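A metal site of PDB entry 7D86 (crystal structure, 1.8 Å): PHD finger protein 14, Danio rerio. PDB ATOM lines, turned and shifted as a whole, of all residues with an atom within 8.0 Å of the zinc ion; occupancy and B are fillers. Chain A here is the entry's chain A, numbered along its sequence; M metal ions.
The backbone carbonyl oxygen of Asn 19 is in hydrogen-bond range of a ring nitrogen (NE2) of His 37 (2.9 Å).
The side-chain sulfur (SG) of Cys 15 sits close to the backbone NH (N) of Gly 17.
The side-chain sulfur of Cys 12 lies close to the backbone NH of Val 14.
N of Cys 12 lies within hydrogen-bond range of O of Gly 17 (2.9 Å).
Four residues have an atom within 4 Å of the zinc ion: Cys 12, Cys 15, His 37 and Cys 40.
The nearest printed residue that does not touch the zinc ion is Val 14 (4.5 Å).
A ring nitrogen (ND1) of His 37 is bound to the zinc ion, 2.1 Å away.
SG of Cys 15 is bound to the zinc ion.
SG of Cys 40 is bound to the zinc ion, 2.3 Å away.
SG of Cys 12 binds the zinc ion.
The zinc ion has four donor atoms within binding distance.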
ATOM      1  N   ILE A  11      -4.948  24.483 -15.765  1.00  0.00           N
ATOM      2  CA  ILE A  11      -6.188  24.002 -16.374  1.00  0.00           C
ATOM      3  C   ILE A  11      -6.752  22.880 -15.526  1.00  0.00           C
ATOM      4  O   ILE A  11      -6.024  21.966 -15.139  1.00  0.00           O
ATOM      5  CB  ILE A  11      -5.961  23.521 -17.817  1.00  0.00           C
ATOM      6  CG1 ILE A  11      -5.350  24.648 -18.647  1.00  0.00           C
ATOM      7  CG2 ILE A  11      -7.286  23.021 -18.434  1.00  0.00           C
ATOM      8  CD1 ILE A  11      -5.004  24.267 -20.058  1.00  0.00           C
ATOM      9  N   CYS A  12      -8.061  22.943 -15.267  1.00  0.00           N
ATOM     10  CA  CYS A  12      -8.778  21.863 -14.606  1.00  0.00           C
ATOM     11  C   CYS A  12      -8.975  20.707 -15.592  1.00  0.00           C
ATOM     12  O   CYS A  12      -9.546  20.897 -16.670  1.00  0.00           O
ATOM     13  CB  CYS A  12     -10.135  22.352 -14.096  1.00  0.00           C
ATOM     14  SG  CYS A  12     -11.105  21.010 -13.399  1.00  0.00           S
ATOM     15  N   CYS A  13      -8.523  19.517 -15.213  1.00  0.00           N
ATOM     16  CA  CYS A  13      -8.626  18.367 -16.107  1.00  0.00           C
ATOM     17  C   CYS A  13     -10.032  17.767 -16.142  1.00  0.00           C
ATOM     18  O   CYS A  13     -10.258  16.806 -16.880  1.00  0.00           O
ATOM     19  CB  CYS A  13      -7.622  17.297 -15.679  1.00  0.00           C
ATOM     20  SG  CYS A  13      -8.123  16.433 -14.194  1.00  0.00           S
ATOM     21  N   VAL A  14     -10.976  18.315 -15.392  1.00  0.00           N
ATOM     22  CA  VAL A  14     -12.355  17.841 -15.425  1.00  0.00           C
ATOM     23  C   VAL A  14     -13.210  18.668 -16.381  1.00  0.00           C
ATOM     24  O   VAL A  14     -13.825  18.128 -17.286  1.00  0.00           O
ATOM     25  CB  VAL A  14     -12.954  17.841 -14.004  1.00  0.00           C
ATOM     26  CG1 VAL A  14     -14.465  17.528 -14.048  1.00  0.00           C
ATOM     27  CG2 VAL A  14     -12.213  16.836 -13.121  1.00  0.00           C
ATOM     28  N   CYS A  15     -13.232  19.992 -16.194  1.00  0.00           N
ATOM     29  CA  CYS A  15     -14.050  20.872 -17.016  1.00  0.00           C
ATOM     30  C   CYS A  15     -13.253  21.596 -18.101  1.00  0.00           C
ATOM     31  O   CYS A  15     -13.877  22.281 -18.923  1.00  0.00           O
ATOM     32  CB  CYS A  15     -14.753  21.905 -16.136  1.00  0.00           C
ATOM     33  SG  CYS A  15     -13.620  23.090 -15.342  1.00  0.00           S
ATOM     34  N   LEU A  16     -11.931  21.468 -18.127  1.00  0.00           N
ATOM     35  CA  LEU A  16     -11.013  22.151 -19.057  1.00  0.00           C
ATOM     36  C   LEU A  16     -11.029  23.669 -18.920  1.00  0.00           C
ATOM     37  O   LEU A  16     -10.436  24.362 -19.744  1.00  0.00           O
ATOM     38  CB  LEU A  16     -11.284  21.763 -20.521  1.00  0.00           C
ATOM     39  CG  LEU A  16     -11.159  20.266 -20.831  1.00  0.00           C
ATOM     40  CD1 LEU A  16     -11.365  19.991 -22.313  1.00  0.00           C
ATOM     41  CD2 LEU A  16      -9.812  19.681 -20.348  1.00  0.00           C
ATOM     42  N   GLY A  17     -11.681  24.217 -17.891  1.00  0.00           N
ATOM     43  CA  GLY A  17     -11.582  25.626 -17.610  1.00  0.00           C
ATOM     44  C   GLY A  17     -10.247  25.977 -16.980  1.00  0.00           C
ATOM     45  O   GLY A  17      -9.477  25.116 -16.546  1.00  0.00           O
ATOM     46  N   ASP A  18      -9.970  27.293 -16.912  1.00  0.00           N
ATOM     47  CA  ASP A  18      -8.688  27.753 -16.390  1.00  0.00           C
ATOM     48  C   ASP A  18      -8.813  28.834 -15.317  1.00  0.00           C
ATOM     49  O   ASP A  18      -7.791  29.393 -14.896  1.00  0.00           O
ATOM     50  CB  ASP A  18      -7.809  28.278 -17.542  1.00  0.00           C
ATOM     51  CG  ASP A  18      -8.480  29.377 -18.353  1.00  0.00           C
ATOM     52  OD1 ASP A  18      -8.907  30.397 -17.776  1.00  0.00           O
ATOM     53  OD2 ASP A  18      -8.544  29.235 -19.591  1.00  0.00           O
ATOM     54  N   ASN A  19     -10.022  29.134 -14.859  1.00  0.00           N
ATOM     55  CA  ASN A  19     -10.205  30.207 -13.889  1.00  0.00           C
ATOM     56  C   ASN A  19      -9.922  29.683 -12.489  1.00  0.00           C
ATOM     57  O   ASN A  19     -10.597  28.766 -12.008  1.00  0.00           O
ATOM     58  CB  ASN A  19     -11.625  30.772 -13.979  1.00  0.00           C
ATOM     59  CG  ASN A  19     -11.728  32.190 -13.460  1.00  0.00           C
ATOM     60  OD1 ASN A  19     -10.711  32.873 -13.286  1.00  0.00           O
ATOM     61  ND2 ASN A  19     -12.951  32.656 -13.212  1.00  0.00           N
ATOM     62  N   ASP A  24     -12.978  28.914  -5.670  1.00  0.00           N
ATOM     63  CA  ASP A  24     -12.650  27.657  -6.324  1.00  0.00           C
ATOM     64  C   ASP A  24     -11.290  27.803  -7.002  1.00  0.00           C
ATOM     65  O   ASP A  24     -11.189  28.341  -8.115  1.00  0.00           O
ATOM     66  CB  ASP A  24     -13.735  27.266  -7.330  1.00  0.00           C
ATOM     67  CG  ASP A  24     -13.621  25.825  -7.775  1.00  0.00           C
ATOM     68  OD1 ASP A  24     -12.684  25.138  -7.316  1.00  0.00           O
ATOM     69  OD2 ASP A  24     -14.474  25.379  -8.562  1.00  0.00           O
ATOM     70  N   GLU A  25     -10.246  27.326  -6.334  1.00  0.00           N
ATOM     71  CA  GLU A  25      -8.897  27.360  -6.885  1.00  0.00           C
ATOM     72  C   GLU A  25      -8.598  26.059  -7.614  1.00  0.00           C
ATOM     73  O   GLU A  25      -9.170  25.019  -7.328  1.00  0.00           O
ATOM     74  CB  GLU A  25      -7.863  27.602  -5.781  1.00  0.00           C
ATOM     75  CG  GLU A  25      -7.944  28.983  -5.148  1.00  0.00           C
ATOM     76  CD  GLU A  25      -6.715  29.329  -4.329  1.00  0.00           C
ATOM     77  OE1 GLU A  25      -6.177  28.428  -3.661  1.00  0.00           O
ATOM     78  OE2 GLU A  25      -6.293  30.499  -4.363  1.00  0.00           O
ATOM     79  N   ILE A  26      -7.678  26.154  -8.571  1.00  0.00           N
ATOM     80  CA  ILE A  26      -7.176  24.975  -9.274  1.00  0.00           C
ATOM     81  C   ILE A  26      -5.983  24.437  -8.487  1.00  0.00           C
ATOM     82  O   ILE A  26      -4.927  25.076  -8.439  1.00  0.00           O
ATOM     83  CB  ILE A  26      -6.801  25.300 -10.722  1.00  0.00           C
ATOM     84  CG1 ILE A  26      -8.057  25.541 -11.562  1.00  0.00           C
ATOM     85  CG2 ILE A  26      -5.940  24.189 -11.328  1.00  0.00           C
ATOM     86  CD1 ILE A  26      -7.786  25.706 -13.046  1.00  0.00           C
ATOM     87  N   THR A  35      -4.193  18.435 -12.301  1.00  0.00           N
ATOM     88  CA  THR A  35      -4.726  19.734 -11.879  1.00  0.00           C
ATOM     89  C   THR A  35      -6.234  19.714 -12.000  1.00  0.00           C
ATOM     90  O   THR A  35      -6.782  19.196 -12.981  1.00  0.00           O
ATOM     91  CB  THR A  35      -4.154  20.869 -12.739  1.00  0.00           C
ATOM     92  OG1 THR A  35      -4.312  20.546 -14.118  1.00  0.00           O
ATOM     93  CG2 THR A  35      -2.668  21.064 -12.430  1.00  0.00           C
ATOM     94  N   VAL A  36      -6.913  20.288 -11.007  1.00  0.00           N
ATOM     95  CA  VAL A  36      -8.372  20.193 -10.930  1.00  0.00           C
ATOM     96  C   VAL A  36      -8.879  21.337 -10.067  1.00  0.00           C
ATOM     97  O   VAL A  36      -8.222  21.773  -9.117  1.00  0.00           O
ATOM     98  CB  VAL A  36      -8.810  18.814 -10.380  1.00  0.00           C
ATOM     99  CG1 VAL A  36      -8.344  18.634  -8.931  1.00  0.00           C
ATOM    100  CG2 VAL A  36     -10.319  18.636 -10.504  1.00  0.00           C
ATOM    101  N   HIS A  37     -10.061  21.865 -10.431  1.00  0.00           N
ATOM    102  CA  HIS A  37     -10.801  22.742  -9.543  1.00  0.00           C
ATOM    103  C   HIS A  37     -11.128  22.012  -8.249  1.00  0.00           C
ATOM    104  O   HIS A  37     -11.520  20.846  -8.268  1.00  0.00           O
ATOM    105  CB  HIS A  37     -12.115  23.206 -10.185  1.00  0.00           C
ATOM    106  CG  HIS A  37     -11.972  24.264 -11.236  1.00  0.00           C
ATOM    107  ND1 HIS A  37     -12.408  24.091 -12.527  1.00  0.00           N
ATOM    108  CD2 HIS A  37     -11.485  25.531 -11.168  1.00  0.00           C
ATOM    109  CE1 HIS A  37     -12.176  25.190 -13.229  1.00  0.00           C
ATOM    110  NE2 HIS A  37     -11.617  26.084 -12.421  1.00  0.00           N
ATOM    111  N   GLU A  38     -10.965  22.711  -7.121  1.00  0.00           N
ATOM    112  CA  GLU A  38     -11.527  22.232  -5.858  1.00  0.00           C
ATOM    113  C   GLU A  38     -12.981  21.805  -6.041  1.00  0.00           C
ATOM    114  O   GLU A  38     -13.373  20.695  -5.641  1.00  0.00           O
ATOM    115  CB  GLU A  38     -11.429  23.327  -4.791  1.00  0.00           C
ATOM    116  CG  GLU A  38     -10.032  23.615  -4.293  1.00  0.00           C
ATOM    117  CD  GLU A  38      -9.983  24.890  -3.460  1.00  0.00           C
ATOM    118  OE1 GLU A  38     -10.789  25.807  -3.738  1.00  0.00           O
ATOM    119  OE2 GLU A  38      -9.141  24.973  -2.548  1.00  0.00           O
ATOM    120  N   GLY A  39     -13.789  22.672  -6.658  1.00  0.00           N
ATOM    121  CA  GLY A  39     -15.203  22.388  -6.844  1.00  0.00           C
ATOM    122  C   GLY A  39     -15.487  21.270  -7.830  1.00  0.00           C
ATOM    123  O   GLY A  39     -16.591  20.714  -7.811  1.00  0.00           O
ATOM    124  N   CYS A  40     -14.522  20.917  -8.682  1.00  0.00           N
ATOM    125  CA  CYS A  40     -14.703  19.788  -9.587  1.00  0.00           C
ATOM    126  C   CYS A  40     -14.232  18.465  -8.992  1.00  0.00           C
ATOM    127  O   CYS A  40     -14.398  17.427  -9.647  1.00  0.00           O
ATOM    128  CB  CYS A  40     -13.972  20.060 -10.907  1.00  0.00           C
ATOM    129  SG  CYS A  40     -14.702  21.363 -11.917  1.00  0.00           S
ATOM    130  N   TYR A  41     -13.680  18.469  -7.782  1.00  0.00           N
ATOM    131  CA  TYR A  41     -13.162  17.244  -7.170  1.00  0.00           C
ATOM    132  C   TYR A  41     -13.747  16.973  -5.793  1.00  0.00           C
ATOM    133  O   TYR A  41     -13.315  16.025  -5.128  1.00  0.00           O
ATOM    134  CB  TYR A  41     -11.626  17.316  -7.058  1.00  0.00           C
ATOM    135  CG  TYR A  41     -10.946  15.967  -6.956  1.00  0.00           C
ATOM    136  CD1 TYR A  41     -11.142  14.996  -7.928  1.00  0.00           C
ATOM    137  CD2 TYR A  41     -10.069  15.675  -5.905  1.00  0.00           C
ATOM    138  CE1 TYR A  41     -10.522  13.776  -7.858  1.00  0.00           C
ATOM    139  CE2 TYR A  41      -9.439  14.445  -5.822  1.00  0.00           C
ATOM    140  CZ  TYR A  41      -9.664  13.509  -6.808  1.00  0.00           C
ATOM    141  OH  TYR A  41      -9.035  12.281  -6.740  1.00  0.00           O
ATOM    142  N   LEU A 100     -19.520  12.156 -14.493  1.00  0.00           N
ATOM    143  CA  LEU A 100     -20.450  13.254 -14.759  1.00  0.00           C
ATOM    144  C   LEU A 100     -21.309  13.001 -15.983  1.00  0.00           C
ATOM    145  O   LEU A 100     -22.410  13.555 -16.094  1.00  0.00           O
ATOM    146  CB  LEU A 100     -19.685  14.561 -14.958  1.00  0.00           C
ATOM    147  CG  LEU A 100     -18.846  14.983 -13.749  1.00  0.00           C
ATOM    148  CD1 LEU A 100     -18.052  16.243 -14.052  1.00  0.00           C
ATOM    149  CD2 LEU A 100     -19.759  15.173 -12.540  1.00  0.00           C
ATOM    150  N   GLU A 170     -20.869  21.822 -20.146  1.00  0.00           N
ATOM    151  CA  GLU A 170     -21.693  21.947 -18.949  1.00  0.00           C
ATOM    152  C   GLU A 170     -22.505  23.224 -19.077  1.00  0.00           C
ATOM    153  O   GLU A 170     -21.926  24.307 -19.256  1.00  0.00           O
ATOM    154  CB  GLU A 170     -20.847  21.965 -17.673  1.00  0.00           C
ATOM    155  CG  GLU A 170     -21.673  22.113 -16.393  1.00  0.00           C
ATOM    156  CD  GLU A 170     -20.819  22.144 -15.131  1.00  0.00           C
ATOM    157  OE1 GLU A 170     -21.389  22.093 -14.030  1.00  0.00           O
ATOM    158  OE2 GLU A 170     -19.577  22.232 -15.252  1.00  0.00           O
HETATM  159 ZN    ZN M   1     -13.059  22.281 -13.267  1.00  0.00          ZN
